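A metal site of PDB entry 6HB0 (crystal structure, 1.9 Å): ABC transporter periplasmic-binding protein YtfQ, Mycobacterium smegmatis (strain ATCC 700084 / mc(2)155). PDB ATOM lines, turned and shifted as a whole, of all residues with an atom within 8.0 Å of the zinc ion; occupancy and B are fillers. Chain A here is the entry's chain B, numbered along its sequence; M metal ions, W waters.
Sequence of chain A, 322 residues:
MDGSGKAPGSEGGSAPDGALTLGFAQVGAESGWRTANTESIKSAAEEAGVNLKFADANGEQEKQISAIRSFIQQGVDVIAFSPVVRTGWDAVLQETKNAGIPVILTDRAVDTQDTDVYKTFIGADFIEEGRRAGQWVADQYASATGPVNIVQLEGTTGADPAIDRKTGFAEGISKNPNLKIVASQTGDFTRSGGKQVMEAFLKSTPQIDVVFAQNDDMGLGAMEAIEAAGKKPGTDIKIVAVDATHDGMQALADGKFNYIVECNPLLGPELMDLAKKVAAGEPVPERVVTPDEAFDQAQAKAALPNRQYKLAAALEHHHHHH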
ATOM      1  N   GLY A 123     -21.870   3.497  -5.468  1.00  0.00           N
ATOM      2  CA  GLY A 123     -20.929   3.843  -6.537  1.00  0.00           C
ATOM      3  C   GLY A 123     -19.508   3.831  -6.000  1.00  0.00           C
ATOM      4  O   GLY A 123     -19.282   3.556  -4.810  1.00  0.00           O
ATOM      5  N   ALA A 124     -18.557   4.062  -6.899  1.00  0.00           N
ATOM      6  CA  ALA A 124     -17.163   4.037  -6.513  1.00  0.00           C
ATOM      7  C   ALA A 124     -16.912   5.298  -5.704  1.00  0.00           C
ATOM      8  O   ALA A 124     -17.502   6.324  -5.969  1.00  0.00           O
ATOM      9  CB  ALA A 124     -16.276   3.986  -7.727  1.00  0.00           C
ATOM     10  N   ASP A 125     -16.027   5.174  -4.750  1.00  0.00           N
ATOM     11  CA  ASP A 125     -15.459   6.275  -3.971  1.00  0.00           C
ATOM     12  C   ASP A 125     -14.077   6.697  -4.541  1.00  0.00           C
ATOM     13  O   ASP A 125     -13.077   6.073  -4.261  1.00  0.00           O
ATOM     14  CB  ASP A 125     -15.278   5.774  -2.564  1.00  0.00           C
ATOM     15  CG  ASP A 125     -14.849   6.882  -1.577  1.00  0.00           C
ATOM     16  OD1 ASP A 125     -14.440   8.009  -2.005  1.00  0.00           O
ATOM     17  OD2 ASP A 125     -14.963   6.577  -0.377  1.00  0.00           O
ATOM     18  N   PHE A 126     -14.069   7.742  -5.346  1.00  0.00           N
ATOM     19  CA  PHE A 126     -12.901   8.152  -6.070  1.00  0.00           C
ATOM     20  C   PHE A 126     -11.864   8.797  -5.124  1.00  0.00           C
ATOM     21  O   PHE A 126     -10.697   8.693  -5.374  1.00  0.00           O
ATOM     22  CB  PHE A 126     -13.291   9.162  -7.132  1.00  0.00           C
ATOM     23  CG  PHE A 126     -14.328   8.661  -8.097  1.00  0.00           C
ATOM     24  CD1 PHE A 126     -14.140   7.483  -8.777  1.00  0.00           C
ATOM     25  CD2 PHE A 126     -15.511   9.398  -8.324  1.00  0.00           C
ATOM     26  CE1 PHE A 126     -15.089   7.019  -9.685  1.00  0.00           C
ATOM     27  CE2 PHE A 126     -16.490   8.923  -9.204  1.00  0.00           C
ATOM     28  CZ  PHE A 126     -16.265   7.738  -9.879  1.00  0.00           C
ATOM     29  N   ILE A 127     -12.303   9.446  -4.056  1.00  0.00           N
ATOM     30  CA  ILE A 127     -11.355   9.978  -3.032  1.00  0.00           C
ATOM     31  C   ILE A 127     -10.597   8.831  -2.447  1.00  0.00           C
ATOM     32  O   ILE A 127      -9.375   8.849  -2.364  1.00  0.00           O
ATOM     33  CB  ILE A 127     -12.053  10.776  -1.922  1.00  0.00           C
ATOM     34  CG1 ILE A 127     -12.720  12.000  -2.540  1.00  0.00           C
ATOM     35  CG2 ILE A 127     -11.046  11.117  -0.821  1.00  0.00           C
ATOM     36  CD1 ILE A 127     -13.288  13.027  -1.557  1.00  0.00           C
ATOM     37  N   GLU A 128     -11.298   7.790  -2.083  1.00  0.00           N
ATOM     38  CA  GLU A 128     -10.680   6.618  -1.487  1.00  0.00           C
ATOM     39  C   GLU A 128      -9.690   5.988  -2.452  1.00  0.00           C
ATOM     40  O   GLU A 128      -8.634   5.526  -2.047  1.00  0.00           O
ATOM     41  CB  GLU A 128     -11.762   5.614  -1.098  1.00  0.00           C
ATOM     42  CG  GLU A 128     -11.297   4.302  -0.554  1.00  0.00           C
ATOM     43  CD  GLU A 128     -11.866   3.171  -1.390  1.00  0.00           C
ATOM     44  OE1 GLU A 128     -12.956   2.689  -1.062  1.00  0.00           O
ATOM     45  OE2 GLU A 128     -11.231   2.769  -2.384  1.00  0.00           O
ATOM     46  N   GLU A 129      -9.996   5.970  -3.754  1.00  0.00           N
ATOM     47  CA  GLU A 129      -9.013   5.436  -4.744  1.00  0.00           C
ATOM     48  C   GLU A 129      -7.727   6.212  -4.701  1.00  0.00           C
ATOM     49  O   GLU A 129      -6.660   5.634  -4.653  1.00  0.00           O
ATOM     50  CB  GLU A 129      -9.529   5.502  -6.206  1.00  0.00           C
ATOM     51  CG  GLU A 129     -10.591   4.486  -6.507  1.00  0.00           C
ATOM     52  CD  GLU A 129     -11.154   4.543  -7.936  1.00  0.00           C
ATOM     53  OE1 GLU A 129     -11.422   5.662  -8.403  1.00  0.00           O
ATOM     54  OE2 GLU A 129     -11.381   3.445  -8.559  1.00  0.00           O
ATOM     55  N   ARG A 131      -6.660   8.107  -2.318  1.00  0.00           N
ATOM     56  CA  ARG A 131      -6.013   7.874  -1.046  1.00  0.00           C
ATOM     57  C   ARG A 131      -5.230   6.596  -0.973  1.00  0.00           C
ATOM     58  O   ARG A 131      -4.120   6.558  -0.433  1.00  0.00           O
ATOM     59  CB  ARG A 131      -7.045   7.899   0.097  1.00  0.00           C
ATOM     60  CG  ARG A 131      -6.406   7.837   1.476  1.00  0.00           C
ATOM     61  CD  ARG A 131      -7.392   8.279   2.539  1.00  0.00           C
ATOM     62  NE  ARG A 131      -8.426   7.322   2.546  1.00  0.00           N
ATOM     63  CZ  ARG A 131      -9.724   7.516   2.402  1.00  0.00           C
ATOM     64  NH1 ARG A 131     -10.302   8.696   2.413  1.00  0.00           N
ATOM     65  NH2 ARG A 131     -10.433   6.422   2.358  1.00  0.00           N
ATOM     66  N   ARG A 132      -5.789   5.519  -1.476  1.00  0.00           N
ATOM     67  CA  ARG A 132      -5.052   4.261  -1.468  1.00  0.00           C
ATOM     68  C   ARG A 132      -3.813   4.295  -2.396  1.00  0.00           C
ATOM     69  O   ARG A 132      -2.773   3.714  -2.081  1.00  0.00           O
ATOM     70  CB  ARG A 132      -6.003   3.109  -1.785  1.00  0.00           C
ATOM     71  CG  ARG A 132      -7.099   2.897  -0.725  1.00  0.00           C
ATOM     72  CD  ARG A 132      -8.384   2.251  -1.310  1.00  0.00           C
ATOM     73  NE  ARG A 132      -7.969   1.063  -1.932  1.00  0.00           N
ATOM     74  CZ  ARG A 132      -8.391   0.504  -3.047  1.00  0.00           C
ATOM     75  NH1 ARG A 132      -9.443   0.915  -3.737  1.00  0.00           N
ATOM     76  NH2 ARG A 132      -7.721  -0.554  -3.425  1.00  0.00           N
ATOM     77  N   GLU A 262      -8.347   0.058  -7.461  1.00  0.00           N
ATOM     78  CA  GLU A 262      -9.665   0.370  -8.024  1.00  0.00           C
ATOM     79  C   GLU A 262     -10.682   0.272  -6.944  1.00  0.00           C
ATOM     80  O   GLU A 262     -10.573  -0.574  -6.113  1.00  0.00           O
ATOM     81  CB  GLU A 262     -10.035  -0.567  -9.175  1.00  0.00           C
ATOM     82  CG  GLU A 262     -11.334  -0.151  -9.821  1.00  0.00           C
ATOM     83  CD  GLU A 262     -11.771  -1.006 -11.013  1.00  0.00           C
ATOM     84  OE1 GLU A 262     -10.930  -1.560 -11.747  1.00  0.00           O
ATOM     85  OE2 GLU A 262     -12.980  -1.032 -11.235  1.00  0.00           O
ATOM     86  N   CYS A 263     -11.646   1.199  -6.950  1.00  0.00           N
ATOM     87  CA  CYS A 263     -12.835   1.084  -6.131  1.00  0.00           C
ATOM     88  C   CYS A 263     -13.916   0.719  -7.120  1.00  0.00           C
ATOM     89  O   CYS A 263     -14.162   1.446  -8.084  1.00  0.00           O
ATOM     90  CB  CYS A 263     -13.155   2.403  -5.444  1.00  0.00           C
ATOM     91  SG  CYS A 263     -14.600   2.270  -4.368  1.00  0.00           S
ATOM     92  N   ASN A 264     -14.561  -0.431  -6.916  1.00  0.00           N
ATOM     93  CA  ASN A 264     -15.561  -0.899  -7.893  1.00  0.00           C
ATOM     94  C   ASN A 264     -16.815  -0.005  -7.991  1.00  0.00           C
ATOM     95  O   ASN A 264     -17.237   0.640  -7.033  1.00  0.00           O
ATOM     96  CB  ASN A 264     -16.069  -2.298  -7.524  1.00  0.00           C
ATOM     97  CG  ASN A 264     -15.033  -3.411  -7.740  1.00  0.00           C
ATOM     98  OD1 ASN A 264     -15.210  -4.481  -7.199  1.00  0.00           O
ATOM     99  ND2 ASN A 264     -13.989  -3.168  -8.528  1.00  0.00           N
ATOM    100  N   PRO A 265     -17.421   0.046  -9.166  1.00  0.00           N
ATOM    101  CA  PRO A 265     -18.761   0.579  -9.239  1.00  0.00           C
ATOM    102  C   PRO A 265     -19.792  -0.383  -8.604  1.00  0.00           C
ATOM    103  O   PRO A 265     -19.430  -1.424  -8.051  1.00  0.00           O
ATOM    104  CB  PRO A 265     -18.973   0.682 -10.752  1.00  0.00           C
ATOM    105  CG  PRO A 265     -18.280  -0.506 -11.270  1.00  0.00           C
ATOM    106  CD  PRO A 265     -17.048  -0.640 -10.408  1.00  0.00           C
ATOM    107  N   ARG A 287     -24.095   5.232   2.053  1.00  0.00           N
ATOM    108  CA  ARG A 287     -23.231   4.882   0.948  1.00  0.00           C
ATOM    109  C   ARG A 287     -22.818   3.444   1.106  1.00  0.00           C
ATOM    110  O   ARG A 287     -22.303   3.062   2.126  1.00  0.00           O
ATOM    111  CB  ARG A 287     -21.991   5.721   1.015  1.00  0.00           C
ATOM    112  CG  ARG A 287     -21.991   6.912   0.098  1.00  0.00           C
ATOM    113  CD  ARG A 287     -21.028   6.570  -1.024  1.00  0.00           C
ATOM    114  NE  ARG A 287     -20.327   7.720  -1.518  1.00  0.00           N
ATOM    115  CZ  ARG A 287     -19.468   7.657  -2.511  1.00  0.00           C
ATOM    116  NH1 ARG A 287     -18.883   8.766  -2.862  1.00  0.00           N
ATOM    117  NH2 ARG A 287     -19.196   6.499  -3.157  1.00  0.00           N
ATOM    118  N   VAL A 288     -23.110   2.628   0.134  1.00  0.00           N
ATOM    119  CA  VAL A 288     -22.635   1.279   0.172  1.00  0.00           C
ATOM    120  C   VAL A 288     -21.143   1.375  -0.062  1.00  0.00           C
ATOM    121  O   VAL A 288     -20.684   2.183  -0.879  1.00  0.00           O
ATOM    122  CB  VAL A 288     -23.301   0.483  -0.935  1.00  0.00           C
ATOM    123  CG1 VAL A 288     -22.630  -0.837  -1.130  1.00  0.00           C
ATOM    124  CG2 VAL A 288     -24.721   0.206  -0.559  1.00  0.00           C
ATOM    125  N   VAL A 289     -20.362   0.546   0.617  1.00  0.00           N
ATOM    126  CA  VAL A 289     -18.962   0.460   0.264  1.00  0.00           C
ATOM    127  C   VAL A 289     -18.782  -0.695  -0.729  1.00  0.00           C
ATOM    128  O   VAL A 289     -19.024  -1.841  -0.385  1.00  0.00           O
ATOM    129  CB  VAL A 289     -18.048   0.323   1.498  1.00  0.00           C
ATOM    130  CG1 VAL A 289     -18.352   1.458   2.512  1.00  0.00           C
ATOM    131  CG2 VAL A 289     -18.185  -1.044   2.094  1.00  0.00           C
ATOM    132  N   THR A 290     -18.405  -0.377  -1.966  1.00  0.00           N
ATOM    133  CA  THR A 290     -18.219  -1.390  -3.001  1.00  0.00           C
ATOM    134  C   THR A 290     -16.895  -2.093  -2.739  1.00  0.00           C
ATOM    135  O   THR A 290     -16.118  -1.633  -1.905  1.00  0.00           O
ATOM    136  CB  THR A 290     -18.201  -0.746  -4.406  1.00  0.00           C
ATOM    137  OG1 THR A 290     -17.257   0.337  -4.441  1.00  0.00           O
ATOM    138  CG2 THR A 290     -19.588  -0.205  -4.732  1.00  0.00           C
ATOM    139  N   PRO A 291     -16.647  -3.219  -3.381  1.00  0.00           N
ATOM    140  CA  PRO A 291     -15.353  -3.870  -3.183  1.00  0.00           C
ATOM    141  C   PRO A 291     -14.196  -3.086  -3.786  1.00  0.00           C
ATOM    142  O   PRO A 291     -14.359  -2.310  -4.779  1.00  0.00           O
ATOM    143  CB  PRO A 291     -15.514  -5.215  -3.911  1.00  0.00           C
ATOM    144  CG  PRO A 291     -16.973  -5.415  -3.964  1.00  0.00           C
ATOM    145  CD  PRO A 291     -17.551  -4.051  -4.180  1.00  0.00           C
ATOM    146  N   ASP A 292     -13.052  -3.282  -3.165  1.00  0.00           N
ATOM    147  CA  ASP A 292     -11.816  -2.659  -3.572  1.00  0.00           C
ATOM    148  C   ASP A 292     -10.854  -3.682  -4.124  1.00  0.00           C
ATOM    149  O   ASP A 292     -10.809  -4.819  -3.691  1.00  0.00           O
ATOM    150  CB  ASP A 292     -11.215  -1.937  -2.365  1.00  0.00           C
ATOM    151  CG  ASP A 292     -11.989  -0.740  -1.965  1.00  0.00           C
ATOM    152  OD1 ASP A 292     -12.639  -0.090  -2.830  1.00  0.00           O
ATOM    153  OD2 ASP A 292     -11.990  -0.412  -0.772  1.00  0.00           O
ATOM    154  N   GLU A 293     -10.115  -3.270  -5.128  1.00  0.00           N
ATOM    155  CA  GLU A 293      -9.097  -4.077  -5.768  1.00  0.00           C
ATOM    156  C   GLU A 293      -7.753  -3.361  -5.624  1.00  0.00           C
ATOM    157  O   GLU A 293      -7.723  -2.118  -5.606  1.00  0.00           O
ATOM    158  CB  GLU A 293      -9.448  -4.229  -7.237  1.00  0.00           C
ATOM    159  CG  GLU A 293     -10.727  -5.015  -7.463  1.00  0.00           C
ATOM    160  CD  GLU A 293     -11.049  -5.312  -8.936  1.00  0.00           C
ATOM    161  OE1 GLU A 293     -10.137  -5.653  -9.725  1.00  0.00           O
ATOM    162  OE2 GLU A 293     -12.232  -5.249  -9.296  1.00  0.00           O
HETATM  163 ZN    ZN M   1     -13.741   1.506  -2.526  1.00  0.00          ZN
HETATM  164  O   HOH W   1     -15.232   0.907  -1.283  1.00  0.00           O
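Residues that only touch the zinc ion: Thr 290. Four residues have an atom within 4 Å of the zinc ion: Glu 128, Cys 263, Thr 290 and Asp 292.
The side-chain carboxylate (OD1) of Asp 125 is in hydrogen-bond range of the backbone NH (N) of Glu 128, at 3.2 Å. OG1 of Thr 290 sits close to SG of Cys 263 (3.3 Å). The side-chain hydroxyl of Thr 290 is in hydrogen-bond range of the backbone carbonyl oxygen of Asn 264 (2.6 Å). N of Cys 263 sits at hydrogen-bond distance from OE2 of Glu 129 (2.8 Å). The guanidinium group (NH1) of Arg 132 sits close to the side-chain carboxylate (OD1) of Asp 292 (3.5 Å). SG of Cys 263 lies close to N of Asp 125, at 3.3 Å. The side-chain carboxylate (OE2) of Glu 128 lies within salt-bridge range of the guanidinium group (NH1) of Arg 132, 2.9 Å away.
The zinc ion is bound by the side-chain carboxylate (OD1) of Asp 292 (2.0 Å), water W1 (2.0 Å), the side-chain carboxylate (OE1) of Glu 128 (2.0 Å) and the side-chain sulfur (SG) of Cys 263 (2.2 Å). Slightly farther from the zinc ion lies OE2 of Glu 128 (2.8 Å).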
